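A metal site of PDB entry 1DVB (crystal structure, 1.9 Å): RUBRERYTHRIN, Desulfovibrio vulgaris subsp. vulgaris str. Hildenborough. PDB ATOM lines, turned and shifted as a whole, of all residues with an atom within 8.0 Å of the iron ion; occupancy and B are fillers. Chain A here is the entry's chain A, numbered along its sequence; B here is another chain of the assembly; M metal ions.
Of the 25 residues printed, 4 come within 4 Å of the iron ion.
The side-chain sulfur of Cys 161 sits close to the backbone NH of Tyr 163 (3.5 Å).
A ring nitrogen (NE2) of His 56 of chain B lies within hydrogen-bond range of the backbone carbonyl oxygen of Cys 161 (2.8 Å).
The backbone carbonyl oxygen (O) of Tyr 163 sits at hydrogen-bond distance from the backbone NH (N) of Cys 158 (2.9 Å).
The side-chain sulfur (SG) of Cys 158 lies close to the backbone NH (N) of Asn 160 (3.4 Å).
SG of Cys 174 lies close to N of Ala 176.
The backbone NH (N) of Cys 174 lies within hydrogen-bond range of the backbone carbonyl oxygen (O) of His 179 (2.5 Å).
The side-chain amide nitrogen of Asn 160 sits close to the side-chain sulfur of Cys 177, 3.2 Å away.
The backbone carbonyl oxygen (O) of Cys 177 lies within hydrogen-bond range of a ring nitrogen (ND1) of His 179, at 3.0 Å.
The iron ion is bound by the side-chain sulfur (SG) of Cys 161.
The iron ion is bound by SG of Cys 158.
The iron ion is bound by the side-chain sulfur (SG) of Cys 174, at 2.3 Å.
SG of Cys 177 is bound to the iron ion (2.3 Å).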
ATOM      1  N   ARG A 157      28.497  12.790  -7.217  1.00  0.00           N
ATOM      2  CA  ARG A 157      27.402  12.155  -7.945  1.00  0.00           C
ATOM      3  C   ARG A 157      26.063  12.662  -7.370  1.00  0.00           C
ATOM      4  O   ARG A 157      25.806  12.837  -6.192  1.00  0.00           O
ATOM      5  CB  ARG A 157      27.553  10.634  -7.908  1.00  0.00           C
ATOM      6  CG  ARG A 157      26.662   9.874  -8.885  1.00  0.00           C
ATOM      7  CD  ARG A 157      26.588   8.392  -8.555  1.00  0.00           C
ATOM      8  NE  ARG A 157      25.948   8.163  -7.252  1.00  0.00           N
ATOM      9  CZ  ARG A 157      25.032   7.225  -7.037  1.00  0.00           C
ATOM     10  NH1 ARG A 157      24.606   6.422  -8.006  1.00  0.00           N
ATOM     11  NH2 ARG A 157      24.465   7.041  -5.844  1.00  0.00           N
ATOM     12  N   CYS A 158      25.186  12.918  -8.319  1.00  0.00           N
ATOM     13  CA  CYS A 158      23.773  13.189  -8.141  1.00  0.00           C
ATOM     14  C   CYS A 158      23.074  11.874  -7.773  1.00  0.00           C
ATOM     15  O   CYS A 158      23.064  10.876  -8.512  1.00  0.00           O
ATOM     16  CB  CYS A 158      23.150  13.754  -9.407  1.00  0.00           C
ATOM     17  SG  CYS A 158      21.430  14.244  -9.139  1.00  0.00           S
ATOM     18  N   ARG A 159      22.479  11.908  -6.562  1.00  0.00           N
ATOM     19  CA  ARG A 159      21.773  10.715  -6.094  1.00  0.00           C
ATOM     20  C   ARG A 159      20.482  10.581  -6.885  1.00  0.00           C
ATOM     21  O   ARG A 159      20.008   9.471  -7.083  1.00  0.00           O
ATOM     22  CB  ARG A 159      21.524  10.805  -4.601  1.00  0.00           C
ATOM     23  CG  ARG A 159      22.886  10.780  -3.895  1.00  0.00           C
ATOM     24  CD  ARG A 159      22.844  10.427  -2.435  1.00  0.00           C
ATOM     25  NE  ARG A 159      22.837   8.916  -2.301  1.00  0.00           N
ATOM     26  CZ  ARG A 159      21.713   8.561  -1.681  1.00  0.00           C
ATOM     27  NH1 ARG A 159      20.969   9.634  -1.387  1.00  0.00           N
ATOM     28  NH2 ARG A 159      21.364   7.343  -1.410  1.00  0.00           N
ATOM     29  N   ASN A 160      19.988  11.734  -7.328  1.00  0.00           N
ATOM     30  CA  ASN A 160      18.687  11.659  -7.985  1.00  0.00           C
ATOM     31  C   ASN A 160      18.731  11.062  -9.388  1.00  0.00           C
ATOM     32  O   ASN A 160      17.815  10.257  -9.705  1.00  0.00           O
ATOM     33  CB  ASN A 160      18.093  13.073  -8.022  1.00  0.00           C
ATOM     34  CG  ASN A 160      16.625  13.029  -8.478  1.00  0.00           C
ATOM     35  OD1 ASN A 160      15.860  12.183  -8.011  1.00  0.00           O
ATOM     36  ND2 ASN A 160      16.335  13.954  -9.389  1.00  0.00           N
ATOM     37  N   CYS A 161      19.748  11.422 -10.194  1.00  0.00           N
ATOM     38  CA  CYS A 161      19.842  10.956 -11.559  1.00  0.00           C
ATOM     39  C   CYS A 161      21.205  10.373 -11.920  1.00  0.00           C
ATOM     40  O   CYS A 161      21.218   9.987 -13.104  1.00  0.00           O
ATOM     41  CB  CYS A 161      19.633  12.033 -12.641  1.00  0.00           C
ATOM     42  SG  CYS A 161      20.899  13.301 -12.704  1.00  0.00           S
ATOM     43  N   GLY A 162      22.202  10.317 -11.071  1.00  0.00           N
ATOM     44  CA  GLY A 162      23.450   9.658 -11.483  1.00  0.00           C
ATOM     45  C   GLY A 162      24.454  10.562 -12.176  1.00  0.00           C
ATOM     46  O   GLY A 162      25.547  10.173 -12.601  1.00  0.00           O
ATOM     47  N   TYR A 163      24.059  11.847 -12.291  1.00  0.00           N
ATOM     48  CA  TYR A 163      24.933  12.742 -13.000  1.00  0.00           C
ATOM     49  C   TYR A 163      26.255  12.859 -12.231  1.00  0.00           C
ATOM     50  O   TYR A 163      26.124  12.991 -11.011  1.00  0.00           O
ATOM     51  CB  TYR A 163      24.358  14.134 -13.130  1.00  0.00           C
ATOM     52  CG  TYR A 163      25.318  15.093 -13.807  1.00  0.00           C
ATOM     53  CD1 TYR A 163      25.632  15.007 -15.161  1.00  0.00           C
ATOM     54  CD2 TYR A 163      25.919  16.110 -13.070  1.00  0.00           C
ATOM     55  CE1 TYR A 163      26.501  15.865 -15.792  1.00  0.00           C
ATOM     56  CE2 TYR A 163      26.787  16.987 -13.689  1.00  0.00           C
ATOM     57  CZ  TYR A 163      27.066  16.846 -15.026  1.00  0.00           C
ATOM     58  OH  TYR A 163      27.935  17.738 -15.584  1.00  0.00           O
ATOM     59  N   VAL A 164      27.348  12.809 -12.981  1.00  0.00           N
ATOM     60  CA  VAL A 164      28.665  12.944 -12.311  1.00  0.00           C
ATOM     61  C   VAL A 164      29.300  14.286 -12.704  1.00  0.00           C
ATOM     62  O   VAL A 164      29.277  14.699 -13.846  1.00  0.00           O
ATOM     63  CB  VAL A 164      29.562  11.733 -12.601  1.00  0.00           C
ATOM     64  CG1 VAL A 164      30.915  11.902 -11.950  1.00  0.00           C
ATOM     65  CG2 VAL A 164      28.925  10.450 -12.083  1.00  0.00           C
ATOM     66  N   PRO A 171      27.613  20.987  -7.651  1.00  0.00           N
ATOM     67  CA  PRO A 171      26.981  22.127  -8.330  1.00  0.00           C
ATOM     68  C   PRO A 171      25.821  22.724  -7.565  1.00  0.00           C
ATOM     69  O   PRO A 171      25.243  22.063  -6.699  1.00  0.00           O
ATOM     70  CB  PRO A 171      26.411  21.478  -9.602  1.00  0.00           C
ATOM     71  CG  PRO A 171      26.293  20.017  -9.339  1.00  0.00           C
ATOM     72  CD  PRO A 171      27.368  19.703  -8.333  1.00  0.00           C
ATOM     73  N   LEU A 173      22.811  23.120  -8.557  1.00  0.00           N
ATOM     74  CA  LEU A 173      21.726  22.580  -9.349  1.00  0.00           C
ATOM     75  C   LEU A 173      22.194  21.453 -10.238  1.00  0.00           C
ATOM     76  O   LEU A 173      23.214  21.583 -10.931  1.00  0.00           O
ATOM     77  CB  LEU A 173      21.188  23.722 -10.202  1.00  0.00           C
ATOM     78  CG  LEU A 173      19.721  23.994 -10.454  1.00  0.00           C
ATOM     79  CD1 LEU A 173      19.438  24.131 -11.947  1.00  0.00           C
ATOM     80  CD2 LEU A 173      18.851  22.889  -9.872  1.00  0.00           C
ATOM     81  N   CYS A 174      21.507  20.321 -10.268  1.00  0.00           N
ATOM     82  CA  CYS A 174      22.032  19.332 -11.198  1.00  0.00           C
ATOM     83  C   CYS A 174      21.718  19.736 -12.650  1.00  0.00           C
ATOM     84  O   CYS A 174      20.583  20.030 -13.084  1.00  0.00           O
ATOM     85  CB  CYS A 174      21.458  17.949 -10.861  1.00  0.00           C
ATOM     86  SG  CYS A 174      22.063  16.658 -11.959  1.00  0.00           S
ATOM     87  N   PRO A 175      22.770  19.781 -13.502  1.00  0.00           N
ATOM     88  CA  PRO A 175      22.597  20.072 -14.918  1.00  0.00           C
ATOM     89  C   PRO A 175      21.688  19.037 -15.614  1.00  0.00           C
ATOM     90  O   PRO A 175      20.963  19.394 -16.541  1.00  0.00           O
ATOM     91  CB  PRO A 175      24.000  19.985 -15.513  1.00  0.00           C
ATOM     92  CG  PRO A 175      24.939  19.651 -14.412  1.00  0.00           C
ATOM     93  CD  PRO A 175      24.177  19.564 -13.124  1.00  0.00           C
ATOM     94  N   ALA A 176      21.729  17.777 -15.182  1.00  0.00           N
ATOM     95  CA  ALA A 176      20.884  16.740 -15.790  1.00  0.00           C
ATOM     96  C   ALA A 176      19.453  16.769 -15.249  1.00  0.00           C
ATOM     97  O   ALA A 176      18.545  16.852 -16.079  1.00  0.00           O
ATOM     98  CB  ALA A 176      21.500  15.347 -15.621  1.00  0.00           C
ATOM     99  N   CYS A 177      19.212  16.694 -13.940  1.00  0.00           N
ATOM    100  CA  CYS A 177      17.855  16.569 -13.413  1.00  0.00           C
ATOM    101  C   CYS A 177      17.367  17.836 -12.773  1.00  0.00           C
ATOM    102  O   CYS A 177      16.196  17.939 -12.377  1.00  0.00           O
ATOM    103  CB  CYS A 177      17.839  15.381 -12.430  1.00  0.00           C
ATOM    104  SG  CYS A 177      18.571  15.785 -10.822  1.00  0.00           S
ATOM    105  N   ALA A 178      18.227  18.855 -12.669  1.00  0.00           N
ATOM    106  CA  ALA A 178      17.796  20.133 -12.101  1.00  0.00           C
ATOM    107  C   ALA A 178      17.349  20.059 -10.643  1.00  0.00           C
ATOM    108  O   ALA A 178      16.641  20.922 -10.096  1.00  0.00           O
ATOM    109  CB  ALA A 178      16.680  20.753 -12.941  1.00  0.00           C
ATOM    110  N   HIS A 179      17.764  19.008  -9.928  1.00  0.00           N
ATOM    111  CA  HIS A 179      17.594  18.978  -8.478  1.00  0.00           C
ATOM    112  C   HIS A 179      18.764  19.749  -7.853  1.00  0.00           C
ATOM    113  O   HIS A 179      19.865  19.943  -8.384  1.00  0.00           O
ATOM    114  CB  HIS A 179      17.461  17.541  -8.022  1.00  0.00           C
ATOM    115  CG  HIS A 179      16.113  16.971  -8.333  1.00  0.00           C
ATOM    116  ND1 HIS A 179      15.557  16.997  -9.594  1.00  0.00           N
ATOM    117  CD2 HIS A 179      15.198  16.350  -7.552  1.00  0.00           C
ATOM    118  CE1 HIS A 179      14.360  16.426  -9.600  1.00  0.00           C
ATOM    119  NE2 HIS A 179      14.123  16.035  -8.366  1.00  0.00           N
ATOM    120  N   PRO A 180      18.567  20.290  -6.659  1.00  0.00           N
ATOM    121  CA  PRO A 180      19.616  21.089  -6.007  1.00  0.00           C
ATOM    122  C   PRO A 180      20.742  20.265  -5.373  1.00  0.00           C
ATOM    123  O   PRO A 180      20.718  19.048  -5.276  1.00  0.00           O
ATOM    124  CB  PRO A 180      18.858  21.821  -4.876  1.00  0.00           C
ATOM    125  CG  PRO A 180      17.557  21.126  -4.707  1.00  0.00           C
ATOM    126  CD  PRO A 180      17.336  20.206  -5.873  1.00  0.00           C
ATOM    127  N   HIS A 183      21.270  16.890  -3.297  1.00  0.00           N
ATOM    128  CA  HIS A 183      21.228  15.529  -3.822  1.00  0.00           C
ATOM    129  C   HIS A 183      22.586  14.920  -4.104  1.00  0.00           C
ATOM    130  O   HIS A 183      22.710  13.713  -4.373  1.00  0.00           O
ATOM    131  CB  HIS A 183      20.358  15.562  -5.110  1.00  0.00           C
ATOM    132  CG  HIS A 183      18.918  15.763  -4.715  1.00  0.00           C
ATOM    133  ND1 HIS A 183      18.073  14.691  -4.513  1.00  0.00           N
ATOM    134  CD2 HIS A 183      18.199  16.882  -4.469  1.00  0.00           C
ATOM    135  CE1 HIS A 183      16.870  15.157  -4.168  1.00  0.00           C
ATOM    136  NE2 HIS A 183      16.909  16.477  -4.137  1.00  0.00           N
ATOM    137  N   PHE A 184      23.610  15.765  -4.050  1.00  0.00           N
ATOM    138  CA  PHE A 184      24.965  15.281  -4.403  1.00  0.00           C
ATOM    139  C   PHE A 184      25.741  14.630  -3.280  1.00  0.00           C
ATOM    140  O   PHE A 184      25.600  14.977  -2.103  1.00  0.00           O
ATOM    141  CB  PHE A 184      25.778  16.489  -4.944  1.00  0.00           C
ATOM    142  CG  PHE A 184      25.408  16.709  -6.418  1.00  0.00           C
ATOM    143  CD1 PHE A 184      26.060  15.976  -7.404  1.00  0.00           C
ATOM    144  CD2 PHE A 184      24.415  17.638  -6.728  1.00  0.00           C
ATOM    145  CE1 PHE A 184      25.729  16.157  -8.732  1.00  0.00           C
ATOM    146  CE2 PHE A 184      24.073  17.828  -8.064  1.00  0.00           C
ATOM    147  CZ  PHE A 184      24.735  17.096  -9.031  1.00  0.00           C
ATOM    148  N   GLN B  52      16.906   6.232 -11.405  1.00  0.00           N
ATOM    149  CA  GLN B  52      17.558   7.378 -12.095  1.00  0.00           C
ATOM    150  C   GLN B  52      17.028   7.500 -13.520  1.00  0.00           C
ATOM    151  O   GLN B  52      16.927   8.609 -14.012  1.00  0.00           O
ATOM    152  CB  GLN B  52      19.071   7.215 -12.018  1.00  0.00           C
ATOM    153  CG  GLN B  52      19.467   7.400 -10.534  1.00  0.00           C
ATOM    154  CD  GLN B  52      20.960   7.197 -10.228  1.00  0.00           C
ATOM    155  OE1 GLN B  52      21.670   6.479 -10.965  1.00  0.00           O
ATOM    156  NE2 GLN B  52      21.414   7.832  -9.154  1.00  0.00           N
ATOM    157  N   GLU B  55      14.110   9.533 -13.627  1.00  0.00           N
ATOM    158  CA  GLU B  55      14.284  10.980 -13.422  1.00  0.00           C
ATOM    159  C   GLU B  55      14.878  11.661 -14.637  1.00  0.00           C
ATOM    160  O   GLU B  55      14.709  12.836 -14.901  1.00  0.00           O
ATOM    161  CB  GLU B  55      15.125  11.167 -12.136  1.00  0.00           C
ATOM    162  CG  GLU B  55      14.476  10.550 -10.893  1.00  0.00           C
ATOM    163  CD  GLU B  55      13.280  11.426 -10.496  1.00  0.00           C
ATOM    164  OE1 GLU B  55      13.402  12.647 -10.657  1.00  0.00           O
ATOM    165  OE2 GLU B  55      12.247  10.882 -10.055  1.00  0.00           O
ATOM    166  N   HIS B  56      15.613  10.954 -15.484  1.00  0.00           N
ATOM    167  CA  HIS B  56      16.016  11.504 -16.763  1.00  0.00           C
ATOM    168  C   HIS B  56      14.736  11.688 -17.611  1.00  0.00           C
ATOM    169  O   HIS B  56      14.538  12.700 -18.257  1.00  0.00           O
ATOM    170  CB  HIS B  56      16.960  10.598 -17.544  1.00  0.00           C
ATOM    171  CG  HIS B  56      18.233  10.306 -16.865  1.00  0.00           C
ATOM    172  ND1 HIS B  56      19.001   9.203 -17.131  1.00  0.00           N
ATOM    173  CD2 HIS B  56      18.898  11.009 -15.913  1.00  0.00           C
ATOM    174  CE1 HIS B  56      20.079   9.230 -16.360  1.00  0.00           C
ATOM    175  NE2 HIS B  56      20.041  10.324 -15.611  1.00  0.00           N
ATOM    176  N   ARG B  59      12.771  14.893 -16.551  1.00  0.00           N
ATOM    177  CA  ARG B  59      13.226  16.199 -17.050  1.00  0.00           C
ATOM    178  C   ARG B  59      12.871  16.359 -18.519  1.00  0.00           C
ATOM    179  O   ARG B  59      12.435  17.425 -18.951  1.00  0.00           O
ATOM    180  CB  ARG B  59      14.739  16.308 -16.852  1.00  0.00           C
ATOM    181  CG  ARG B  59      15.420  17.569 -17.313  1.00  0.00           C
ATOM    182  CD  ARG B  59      15.030  18.792 -16.530  1.00  0.00           C
ATOM    183  NE  ARG B  59      15.900  19.916 -16.468  1.00  0.00           N
ATOM    184  CZ  ARG B  59      17.191  20.162 -16.571  1.00  0.00           C
ATOM    185  NH1 ARG B  59      18.080  19.205 -16.771  1.00  0.00           N
ATOM    186  NH2 ARG B  59      17.621  21.416 -16.451  1.00  0.00           N
ATOM    187  N   SER B 123      24.155  16.333 -20.500  1.00  0.00           N
ATOM    188  CA  SER B 123      24.346  15.933 -19.093  1.00  0.00           C
ATOM    189  C   SER B 123      23.871  14.537 -18.861  1.00  0.00           C
ATOM    190  O   SER B 123      24.544  13.716 -18.239  1.00  0.00           O
ATOM    191  CB  SER B 123      23.614  16.963 -18.251  1.00  0.00           C
ATOM    192  OG  SER B 123      24.272  18.173 -18.606  1.00  0.00           O
ATOM    193  N   ALA B 127      25.709  10.700 -17.214  1.00  0.00           N
ATOM    194  CA  ALA B 127      25.151   9.714 -16.295  1.00  0.00           C
ATOM    195  C   ALA B 127      25.147   8.345 -16.923  1.00  0.00           C
ATOM    196  O   ALA B 127      25.454   7.351 -16.269  1.00  0.00           O
ATOM    197  CB  ALA B 127      23.709  10.064 -15.878  1.00  0.00           C
HETATM  198 FE    FE M   1      20.719  14.936 -11.205  1.00  0.00          FE
